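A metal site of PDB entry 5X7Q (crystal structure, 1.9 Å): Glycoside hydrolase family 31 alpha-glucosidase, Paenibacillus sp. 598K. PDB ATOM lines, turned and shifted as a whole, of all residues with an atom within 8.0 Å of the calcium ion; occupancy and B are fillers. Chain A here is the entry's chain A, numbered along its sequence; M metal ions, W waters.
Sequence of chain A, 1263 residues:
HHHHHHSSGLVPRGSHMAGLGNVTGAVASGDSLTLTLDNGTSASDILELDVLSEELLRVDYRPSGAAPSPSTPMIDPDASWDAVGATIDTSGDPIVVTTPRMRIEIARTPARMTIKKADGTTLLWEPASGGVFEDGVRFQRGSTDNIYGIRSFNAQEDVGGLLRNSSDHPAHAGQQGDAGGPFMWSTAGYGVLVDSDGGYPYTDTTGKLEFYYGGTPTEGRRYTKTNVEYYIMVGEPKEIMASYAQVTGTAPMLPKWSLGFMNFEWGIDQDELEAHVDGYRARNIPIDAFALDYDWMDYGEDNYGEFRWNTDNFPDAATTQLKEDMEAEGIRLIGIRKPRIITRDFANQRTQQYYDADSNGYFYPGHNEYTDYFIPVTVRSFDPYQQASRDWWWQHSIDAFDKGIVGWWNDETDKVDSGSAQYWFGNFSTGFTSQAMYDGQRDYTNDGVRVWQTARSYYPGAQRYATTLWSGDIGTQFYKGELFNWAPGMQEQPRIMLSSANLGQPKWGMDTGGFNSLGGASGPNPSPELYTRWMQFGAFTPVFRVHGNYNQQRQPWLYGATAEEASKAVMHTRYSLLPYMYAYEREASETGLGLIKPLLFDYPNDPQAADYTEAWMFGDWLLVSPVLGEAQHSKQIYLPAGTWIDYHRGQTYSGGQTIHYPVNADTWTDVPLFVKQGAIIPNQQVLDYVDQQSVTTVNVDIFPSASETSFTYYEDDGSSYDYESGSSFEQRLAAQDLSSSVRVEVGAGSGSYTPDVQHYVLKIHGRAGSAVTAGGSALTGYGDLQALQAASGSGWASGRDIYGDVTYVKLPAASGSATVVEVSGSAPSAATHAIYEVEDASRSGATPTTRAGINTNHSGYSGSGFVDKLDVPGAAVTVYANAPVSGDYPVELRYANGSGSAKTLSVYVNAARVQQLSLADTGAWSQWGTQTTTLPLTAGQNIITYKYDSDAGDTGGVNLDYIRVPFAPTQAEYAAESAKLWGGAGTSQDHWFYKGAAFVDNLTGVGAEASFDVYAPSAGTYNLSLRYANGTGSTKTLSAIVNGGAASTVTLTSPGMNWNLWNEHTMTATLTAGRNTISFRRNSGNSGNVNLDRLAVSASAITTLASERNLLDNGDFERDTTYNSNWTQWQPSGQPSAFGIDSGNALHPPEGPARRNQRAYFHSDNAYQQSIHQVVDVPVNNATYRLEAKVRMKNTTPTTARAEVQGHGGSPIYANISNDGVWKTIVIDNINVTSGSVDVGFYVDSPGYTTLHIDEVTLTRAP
The guanidinium group (NE) of Arg 1155 lies within salt-bridge range of the side-chain carboxylate (OE2) of Glu 1256 (2.8 Å).
The side-chain carboxylate (OD1) of Asp 666 lies within salt-bridge range of the guanidinium group (NH2) of Arg 1155 (2.8 Å).
The backbone NH of Ala 1154 lies close to the side-chain carboxylate of Asp 1255, at 2.8 Å.
NE2 of Gln 1158 lies within hydrogen-bond range of O of Arg 1119 (2.9 Å).
The side-chain amide oxygen (OD1) of Asn 1114 lies within hydrogen-bond range of the backbone NH (N) of Glu 1118 (3.1 Å).
The side-chain amide nitrogen (NE2) of Gln 1158 is in hydrogen-bond range of the backbone carbonyl oxygen (O) of Phe 1117, at 2.8 Å.
OE1 of Glu 1118 sits at hydrogen-bond distance from N of Asn 1157, at 2.9 Å.
NH1 of Arg 1156 is in salt-bridge range of OE1 of Glu 1118.
Within 4 Å of the calcium ion: Asp 1116, Glu 1118, Arg 1155, Gln 1158 and Asp 1255.
The nearest printed residue that does not touch the calcium ion is Pro 1153 (4.4 Å).
The calcium ion is bound by water W1 (2.2 Å), the side-chain carboxylate (OE2) of Glu 1118 (2.3 Å), the side-chain carboxylate (OD1) of Asp 1255 (2.3 Å), the backbone carbonyl oxygen (O) of Gln 1158 (2.4 Å), the backbone carbonyl oxygen (O) of Asp 1116 (2.5 Å), the side-chain carboxylate (OD2) of Asp 1255 (2.8 Å) and the backbone carbonyl oxygen (O) of Arg 1155 (2.8 Å).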
ATOM      1  N   THR A 562      -1.648  20.914  23.210  1.00  0.00           N
ATOM      2  CA  THR A 562      -1.428  21.746  24.388  1.00  0.00           C
ATOM      3  C   THR A 562      -0.379  22.822  24.098  1.00  0.00           C
ATOM      4  O   THR A 562      -0.619  24.008  24.325  1.00  0.00           O
ATOM      5  CB  THR A 562      -1.030  20.947  25.620  1.00  0.00           C
ATOM      6  OG1 THR A 562      -2.021  19.953  25.861  1.00  0.00           O
ATOM      7  CG2 THR A 562      -0.922  21.867  26.820  1.00  0.00           C
ATOM      8  N   ASP A 666      -1.688  19.139  34.533  1.00  0.00           N
ATOM      9  CA  ASP A 666      -2.370  18.439  33.434  1.00  0.00           C
ATOM     10  C   ASP A 666      -2.628  19.307  32.189  1.00  0.00           C
ATOM     11  O   ASP A 666      -2.474  18.831  31.059  1.00  0.00           O
ATOM     12  CB  ASP A 666      -3.672  17.856  33.954  1.00  0.00           C
ATOM     13  CG  ASP A 666      -4.312  16.917  32.968  1.00  0.00           C
ATOM     14  OD1 ASP A 666      -3.618  16.216  32.199  1.00  0.00           O
ATOM     15  OD2 ASP A 666      -5.542  16.866  33.004  1.00  0.00           O
ATOM     16  N   ASN A1114      -4.742   6.056  32.801  1.00  0.00           N
ATOM     17  CA  ASN A1114      -3.664   6.476  31.904  1.00  0.00           C
ATOM     18  C   ASN A1114      -4.089   6.420  30.429  1.00  0.00           C
ATOM     19  O   ASN A1114      -3.320   6.011  29.545  1.00  0.00           O
ATOM     20  CB  ASN A1114      -2.406   5.641  32.148  1.00  0.00           C
ATOM     21  CG  ASN A1114      -1.136   6.260  31.563  1.00  0.00           C
ATOM     22  OD1 ASN A1114      -0.948   7.473  31.591  1.00  0.00           O
ATOM     23  ND2 ASN A1114      -0.263   5.410  31.069  1.00  0.00           N
ATOM     24  N   GLY A1115      -5.323   6.870  30.176  1.00  0.00           N
ATOM     25  CA  GLY A1115      -5.901   6.896  28.860  1.00  0.00           C
ATOM     26  C   GLY A1115      -5.169   7.854  27.945  1.00  0.00           C
ATOM     27  O   GLY A1115      -5.177   7.675  26.724  1.00  0.00           O
ATOM     28  N   ASP A1116      -4.559   8.894  28.538  1.00  0.00           N
ATOM     29  CA  ASP A1116      -3.774   9.891  27.810  1.00  0.00           C
ATOM     30  C   ASP A1116      -2.256   9.609  27.737  1.00  0.00           C
ATOM     31  O   ASP A1116      -1.500  10.429  27.199  1.00  0.00           O
ATOM     32  CB  ASP A1116      -4.032  11.281  28.408  1.00  0.00           C
ATOM     33  CG  ASP A1116      -3.715  11.381  29.895  1.00  0.00           C
ATOM     34  OD1 ASP A1116      -3.116  10.437  30.479  1.00  0.00           O
ATOM     35  OD2 ASP A1116      -4.079  12.406  30.491  1.00  0.00           O
ATOM     36  N   PHE A1117      -1.842   8.458  28.294  1.00  0.00           N
ATOM     37  CA  PHE A1117      -0.443   8.005  28.340  1.00  0.00           C
ATOM     38  C   PHE A1117       0.510   9.058  28.953  1.00  0.00           C
ATOM     39  O   PHE A1117       1.697   9.080  28.650  1.00  0.00           O
ATOM     40  CB  PHE A1117       0.035   7.562  26.956  1.00  0.00           C
ATOM     41  CG  PHE A1117      -0.898   6.573  26.299  1.00  0.00           C
ATOM     42  CD1 PHE A1117      -0.895   5.243  26.673  1.00  0.00           C
ATOM     43  CD2 PHE A1117      -1.792   7.000  25.329  1.00  0.00           C
ATOM     44  CE1 PHE A1117      -1.775   4.333  26.082  1.00  0.00           C
ATOM     45  CE2 PHE A1117      -2.676   6.101  24.746  1.00  0.00           C
ATOM     46  CZ  PHE A1117      -2.665   4.768  25.115  1.00  0.00           C
ATOM     47  N   GLU A1118      -0.017   9.907  29.842  1.00  0.00           N
ATOM     48  CA  GLU A1118       0.775  11.004  30.401  1.00  0.00           C
ATOM     49  C   GLU A1118       1.643  10.603  31.566  1.00  0.00           C
ATOM     50  O   GLU A1118       2.542  11.354  31.957  1.00  0.00           O
ATOM     51  CB  GLU A1118      -0.124  12.162  30.798  1.00  0.00           C
ATOM     52  CG  GLU A1118      -0.725  12.848  29.591  1.00  0.00           C
ATOM     53  CD  GLU A1118       0.352  13.362  28.659  1.00  0.00           C
ATOM     54  OE1 GLU A1118       1.317  13.998  29.135  1.00  0.00           O
ATOM     55  OE2 GLU A1118       0.259  13.115  27.445  1.00  0.00           O
ATOM     56  N   ARG A1119       1.400   9.421  32.129  1.00  0.00           N
ATOM     57  CA  ARG A1119       2.143   8.951  33.289  1.00  0.00           C
ATOM     58  C   ARG A1119       3.620   8.774  32.922  1.00  0.00           C
ATOM     59  O   ARG A1119       3.971   8.320  31.807  1.00  0.00           O
ATOM     60  CB  ARG A1119       1.570   7.644  33.808  1.00  0.00           C
ATOM     61  CG  ARG A1119       2.150   7.166  35.135  1.00  0.00           C
ATOM     62  CD  ARG A1119       1.327   6.052  35.784  1.00  0.00           C
ATOM     63  NE  ARG A1119      -0.044   6.479  35.983  1.00  0.00           N
ATOM     64  CZ  ARG A1119      -1.131   5.707  35.934  1.00  0.00           C
ATOM     65  NH1 ARG A1119      -1.043   4.392  35.777  1.00  0.00           N
ATOM     66  NH2 ARG A1119      -2.328   6.268  36.082  1.00  0.00           N
ATOM     67  N   ILE A1141       5.735   4.304  24.814  1.00  0.00           N
ATOM     68  CA  ILE A1141       5.128   5.605  25.114  1.00  0.00           C
ATOM     69  C   ILE A1141       6.246   6.612  25.209  1.00  0.00           C
ATOM     70  O   ILE A1141       7.172   6.434  25.975  1.00  0.00           O
ATOM     71  CB  ILE A1141       4.389   5.577  26.472  1.00  0.00           C
ATOM     72  CG1 ILE A1141       3.218   4.575  26.432  1.00  0.00           C
ATOM     73  CG2 ILE A1141       3.899   6.979  26.863  1.00  0.00           C
ATOM     74  CD1 ILE A1141       2.592   4.317  27.780  1.00  0.00           C
ATOM     75  N   ASP A1142       6.172   7.669  24.413  1.00  0.00           N
ATOM     76  CA  ASP A1142       7.086   8.813  24.572  1.00  0.00           C
ATOM     77  C   ASP A1142       6.486  10.068  23.919  1.00  0.00           C
ATOM     78  O   ASP A1142       5.324  10.054  23.520  1.00  0.00           O
ATOM     79  CB  ASP A1142       8.527   8.487  24.120  1.00  0.00           C
ATOM     80  CG  ASP A1142       8.647   8.158  22.633  1.00  0.00           C
ATOM     81  OD1 ASP A1142       8.069   8.878  21.770  1.00  0.00           O
ATOM     82  OD2 ASP A1142       9.379   7.179  22.332  1.00  0.00           O
ATOM     83  N   GLY A1152       4.498  14.754  17.515  1.00  0.00           N
ATOM     84  CA  GLY A1152       4.083  15.021  18.896  1.00  0.00           C
ATOM     85  C   GLY A1152       2.862  14.266  19.376  1.00  0.00           C
ATOM     86  O   GLY A1152       2.292  13.439  18.642  1.00  0.00           O
ATOM     87  N   PRO A1153       2.448  14.520  20.624  1.00  0.00           N
ATOM     88  CA  PRO A1153       1.222  13.932  21.163  1.00  0.00           C
ATOM     89  C   PRO A1153       0.015  14.695  20.658  1.00  0.00           C
ATOM     90  O   PRO A1153       0.166  15.772  20.086  1.00  0.00           O
ATOM     91  CB  PRO A1153       1.396  14.086  22.677  1.00  0.00           C
ATOM     92  CG  PRO A1153       2.199  15.321  22.813  1.00  0.00           C
ATOM     93  CD  PRO A1153       3.085  15.431  21.597  1.00  0.00           C
ATOM     94  N   ALA A1154      -1.185  14.151  20.862  1.00  0.00           N
ATOM     95  CA  ALA A1154      -2.410  14.905  20.544  1.00  0.00           C
ATOM     96  C   ALA A1154      -2.662  15.969  21.621  1.00  0.00           C
ATOM     97  O   ALA A1154      -3.088  17.082  21.328  1.00  0.00           O
ATOM     98  CB  ALA A1154      -3.597  13.984  20.422  1.00  0.00           C
ATOM     99  N   ARG A1155      -2.370  15.612  22.870  1.00  0.00           N
ATOM    100  CA  ARG A1155      -2.486  16.555  23.993  1.00  0.00           C
ATOM    101  C   ARG A1155      -1.377  16.292  25.006  1.00  0.00           C
ATOM    102  O   ARG A1155      -0.938  15.150  25.199  1.00  0.00           O
ATOM    103  CB  ARG A1155      -3.864  16.430  24.681  1.00  0.00           C
ATOM    104  CG  ARG A1155      -4.207  17.604  25.620  1.00  0.00           C
ATOM    105  CD  ARG A1155      -5.437  17.313  26.503  1.00  0.00           C
ATOM    106  NE  ARG A1155      -5.121  16.302  27.519  1.00  0.00           N
ATOM    107  CZ  ARG A1155      -4.485  16.543  28.678  1.00  0.00           C
ATOM    108  NH1 ARG A1155      -4.092  17.767  29.015  1.00  0.00           N
ATOM    109  NH2 ARG A1155      -4.224  15.543  29.498  1.00  0.00           N
ATOM    110  N   ARG A1156      -0.945  17.364  25.638  1.00  0.00           N
ATOM    111  CA  ARG A1156       0.032  17.334  26.715  1.00  0.00           C
ATOM    112  C   ARG A1156       1.386  16.792  26.234  1.00  0.00           C
ATOM    113  O   ARG A1156       1.899  17.314  25.238  1.00  0.00           O
ATOM    114  CB  ARG A1156      -0.562  16.675  27.985  1.00  0.00           C
ATOM    115  CG  ARG A1156       0.167  17.116  29.244  1.00  0.00           C
ATOM    116  CD  ARG A1156      -0.343  16.483  30.533  1.00  0.00           C
ATOM    117  NE  ARG A1156       0.479  16.938  31.665  1.00  0.00           N
ATOM    118  CZ  ARG A1156       1.612  16.354  32.073  1.00  0.00           C
ATOM    119  NH1 ARG A1156       2.113  15.274  31.462  1.00  0.00           N
ATOM    120  NH2 ARG A1156       2.276  16.869  33.100  1.00  0.00           N
ATOM    121  N   ASN A1157       1.964  15.794  26.903  1.00  0.00           N
ATOM    122  CA  ASN A1157       3.389  15.487  26.721  1.00  0.00           C
ATOM    123  C   ASN A1157       3.678  14.202  25.978  1.00  0.00           C
ATOM    124  O   ASN A1157       4.701  14.106  25.324  1.00  0.00           O
ATOM    125  CB  ASN A1157       4.100  15.422  28.078  1.00  0.00           C
ATOM    126  CG  ASN A1157       5.574  15.837  27.999  1.00  0.00           C
ATOM    127  OD1 ASN A1157       5.951  16.689  27.220  1.00  0.00           O
ATOM    128  ND2 ASN A1157       6.403  15.229  28.844  1.00  0.00           N
ATOM    129  N   GLN A1158       2.798  13.197  26.072  1.00  0.00           N
ATOM    130  CA  GLN A1158       3.122  11.860  25.605  1.00  0.00           C
ATOM    131  C   GLN A1158       1.986  11.190  24.810  1.00  0.00           C
ATOM    132  O   GLN A1158       0.802  11.528  24.926  1.00  0.00           O
ATOM    133  CB  GLN A1158       3.520  10.972  26.794  1.00  0.00           C
ATOM    134  CG  GLN A1158       4.811  11.407  27.504  1.00  0.00           C
ATOM    135  CD  GLN A1158       5.228  10.507  28.669  1.00  0.00           C
ATOM    136  OE1 GLN A1158       6.406  10.458  28.996  1.00  0.00           O
ATOM    137  NE2 GLN A1158       4.277   9.793  29.288  1.00  0.00           N
ATOM    138  N   ARG A1159       2.361  10.203  24.020  1.00  0.00           N
ATOM    139  CA  ARG A1159       1.377   9.371  23.305  1.00  0.00           C
ATOM    140  C   ARG A1159       1.963   7.985  23.110  1.00  0.00           C
ATOM    141  O   ARG A1159       3.199   7.807  23.031  1.00  0.00           O
ATOM    142  CB  ARG A1159       0.957  10.019  21.972  1.00  0.00           C
ATOM    143  CG  ARG A1159       1.998   9.975  20.839  1.00  0.00           C
ATOM    144  CD  ARG A1159       3.222  10.841  21.074  1.00  0.00           C
ATOM    145  NE  ARG A1159       4.148  10.869  19.945  1.00  0.00           N
ATOM    146  CZ  ARG A1159       5.033   9.902  19.645  1.00  0.00           C
ATOM    147  NH1 ARG A1159       5.148   8.816  20.402  1.00  0.00           N
ATOM    148  NH2 ARG A1159       5.832  10.056  18.584  1.00  0.00           N
ATOM    149  N   ALA A1160       1.090   7.000  23.038  1.00  0.00           N
ATOM    150  CA  ALA A1160       1.512   5.670  22.727  1.00  0.00           C
ATOM    151  C   ALA A1160       1.916   5.601  21.249  1.00  0.00           C
ATOM    152  O   ALA A1160       1.409   6.360  20.416  1.00  0.00           O
ATOM    153  CB  ALA A1160       0.404   4.670  23.039  1.00  0.00           C
ATOM    154  N   TRP A1223      -3.745  13.659  13.050  1.00  0.00           N
ATOM    155  CA  TRP A1223      -4.541  13.191  14.189  1.00  0.00           C
ATOM    156  C   TRP A1223      -6.019  13.183  13.817  1.00  0.00           C
ATOM    157  O   TRP A1223      -6.538  14.202  13.383  1.00  0.00           O
ATOM    158  CB  TRP A1223      -4.335  14.080  15.423  1.00  0.00           C
ATOM    159  CG  TRP A1223      -3.062  13.832  16.144  1.00  0.00           C
ATOM    160  CD1 TRP A1223      -1.995  14.682  16.225  1.00  0.00           C
ATOM    161  CD2 TRP A1223      -2.724  12.688  16.949  1.00  0.00           C
ATOM    162  NE1 TRP A1223      -1.005  14.123  17.018  1.00  0.00           N
ATOM    163  CE2 TRP A1223      -1.423  12.907  17.471  1.00  0.00           C
ATOM    164  CE3 TRP A1223      -3.387  11.510  17.271  1.00  0.00           C
ATOM    165  CZ2 TRP A1223      -0.782  11.988  18.297  1.00  0.00           C
ATOM    166  CZ3 TRP A1223      -2.750  10.583  18.094  1.00  0.00           C
ATOM    167  CH2 TRP A1223      -1.459  10.835  18.600  1.00  0.00           C
ATOM    168  N   ILE A1254      -1.438   6.746  19.322  1.00  0.00           N
ATOM    169  CA  ILE A1254      -2.690   6.676  20.052  1.00  0.00           C
ATOM    170  C   ILE A1254      -2.571   7.620  21.236  1.00  0.00           C
ATOM    171  O   ILE A1254      -1.564   7.587  21.942  1.00  0.00           O
ATOM    172  CB  ILE A1254      -2.973   5.272  20.613  1.00  0.00           C
ATOM    173  CG1 ILE A1254      -2.812   4.171  19.560  1.00  0.00           C
ATOM    174  CG2 ILE A1254      -4.365   5.224  21.226  1.00  0.00           C
ATOM    175  CD1 ILE A1254      -2.543   2.808  20.155  1.00  0.00           C
ATOM    176  N   ASP A1255      -3.605   8.426  21.461  1.00  0.00           N
ATOM    177  CA  ASP A1255      -3.610   9.366  22.581  1.00  0.00           C
ATOM    178  C   ASP A1255      -5.035   9.705  23.010  1.00  0.00           C
ATOM    179  O   ASP A1255      -5.992   9.467  22.260  1.00  0.00           O
ATOM    180  CB  ASP A1255      -2.868  10.637  22.151  1.00  0.00           C
ATOM    181  CG  ASP A1255      -2.333  11.438  23.314  1.00  0.00           C
ATOM    182  OD1 ASP A1255      -2.485  10.985  24.478  1.00  0.00           O
ATOM    183  OD2 ASP A1255      -1.786  12.513  23.074  1.00  0.00           O
ATOM    184  N   GLU A1256      -5.167  10.276  24.202  1.00  0.00           N
ATOM    185  CA  GLU A1256      -6.424  10.829  24.690  1.00  0.00           C
ATOM    186  C   GLU A1256      -7.584   9.818  24.631  1.00  0.00           C
ATOM    187  O   GLU A1256      -8.680  10.144  24.190  1.00  0.00           O
ATOM    188  CB  GLU A1256      -6.764  12.089  23.884  1.00  0.00           C
ATOM    189  CG  GLU A1256      -5.825  13.248  24.135  1.00  0.00           C
ATOM    190  CD  GLU A1256      -6.166  13.928  25.449  1.00  0.00           C
ATOM    191  OE1 GLU A1256      -7.219  14.632  25.526  1.00  0.00           O
ATOM    192  OE2 GLU A1256      -5.412  13.703  26.411  1.00  0.00           O
ATOM    193  N   VAL A1257      -7.339   8.605  25.086  1.00  0.00           N
ATOM    194  CA  VAL A1257      -8.353   7.558  25.042  1.00  0.00           C
ATOM    195  C   VAL A1257      -9.285   7.748  26.244  1.00  0.00           C
ATOM    196  O   VAL A1257      -8.808   7.874  27.377  1.00  0.00           O
ATOM    197  CB  VAL A1257      -7.753   6.157  25.079  1.00  0.00           C
ATOM    198  CG1 VAL A1257      -8.815   5.116  24.810  1.00  0.00           C
ATOM    199  CG2 VAL A1257      -6.610   6.040  24.062  1.00  0.00           C
HETATM  200 CA    CA M   1      -1.226  12.461  25.775  1.00  0.00          CA
HETATM  201  O   HOH W   1      -2.863  13.724  26.457  1.00  0.00           O
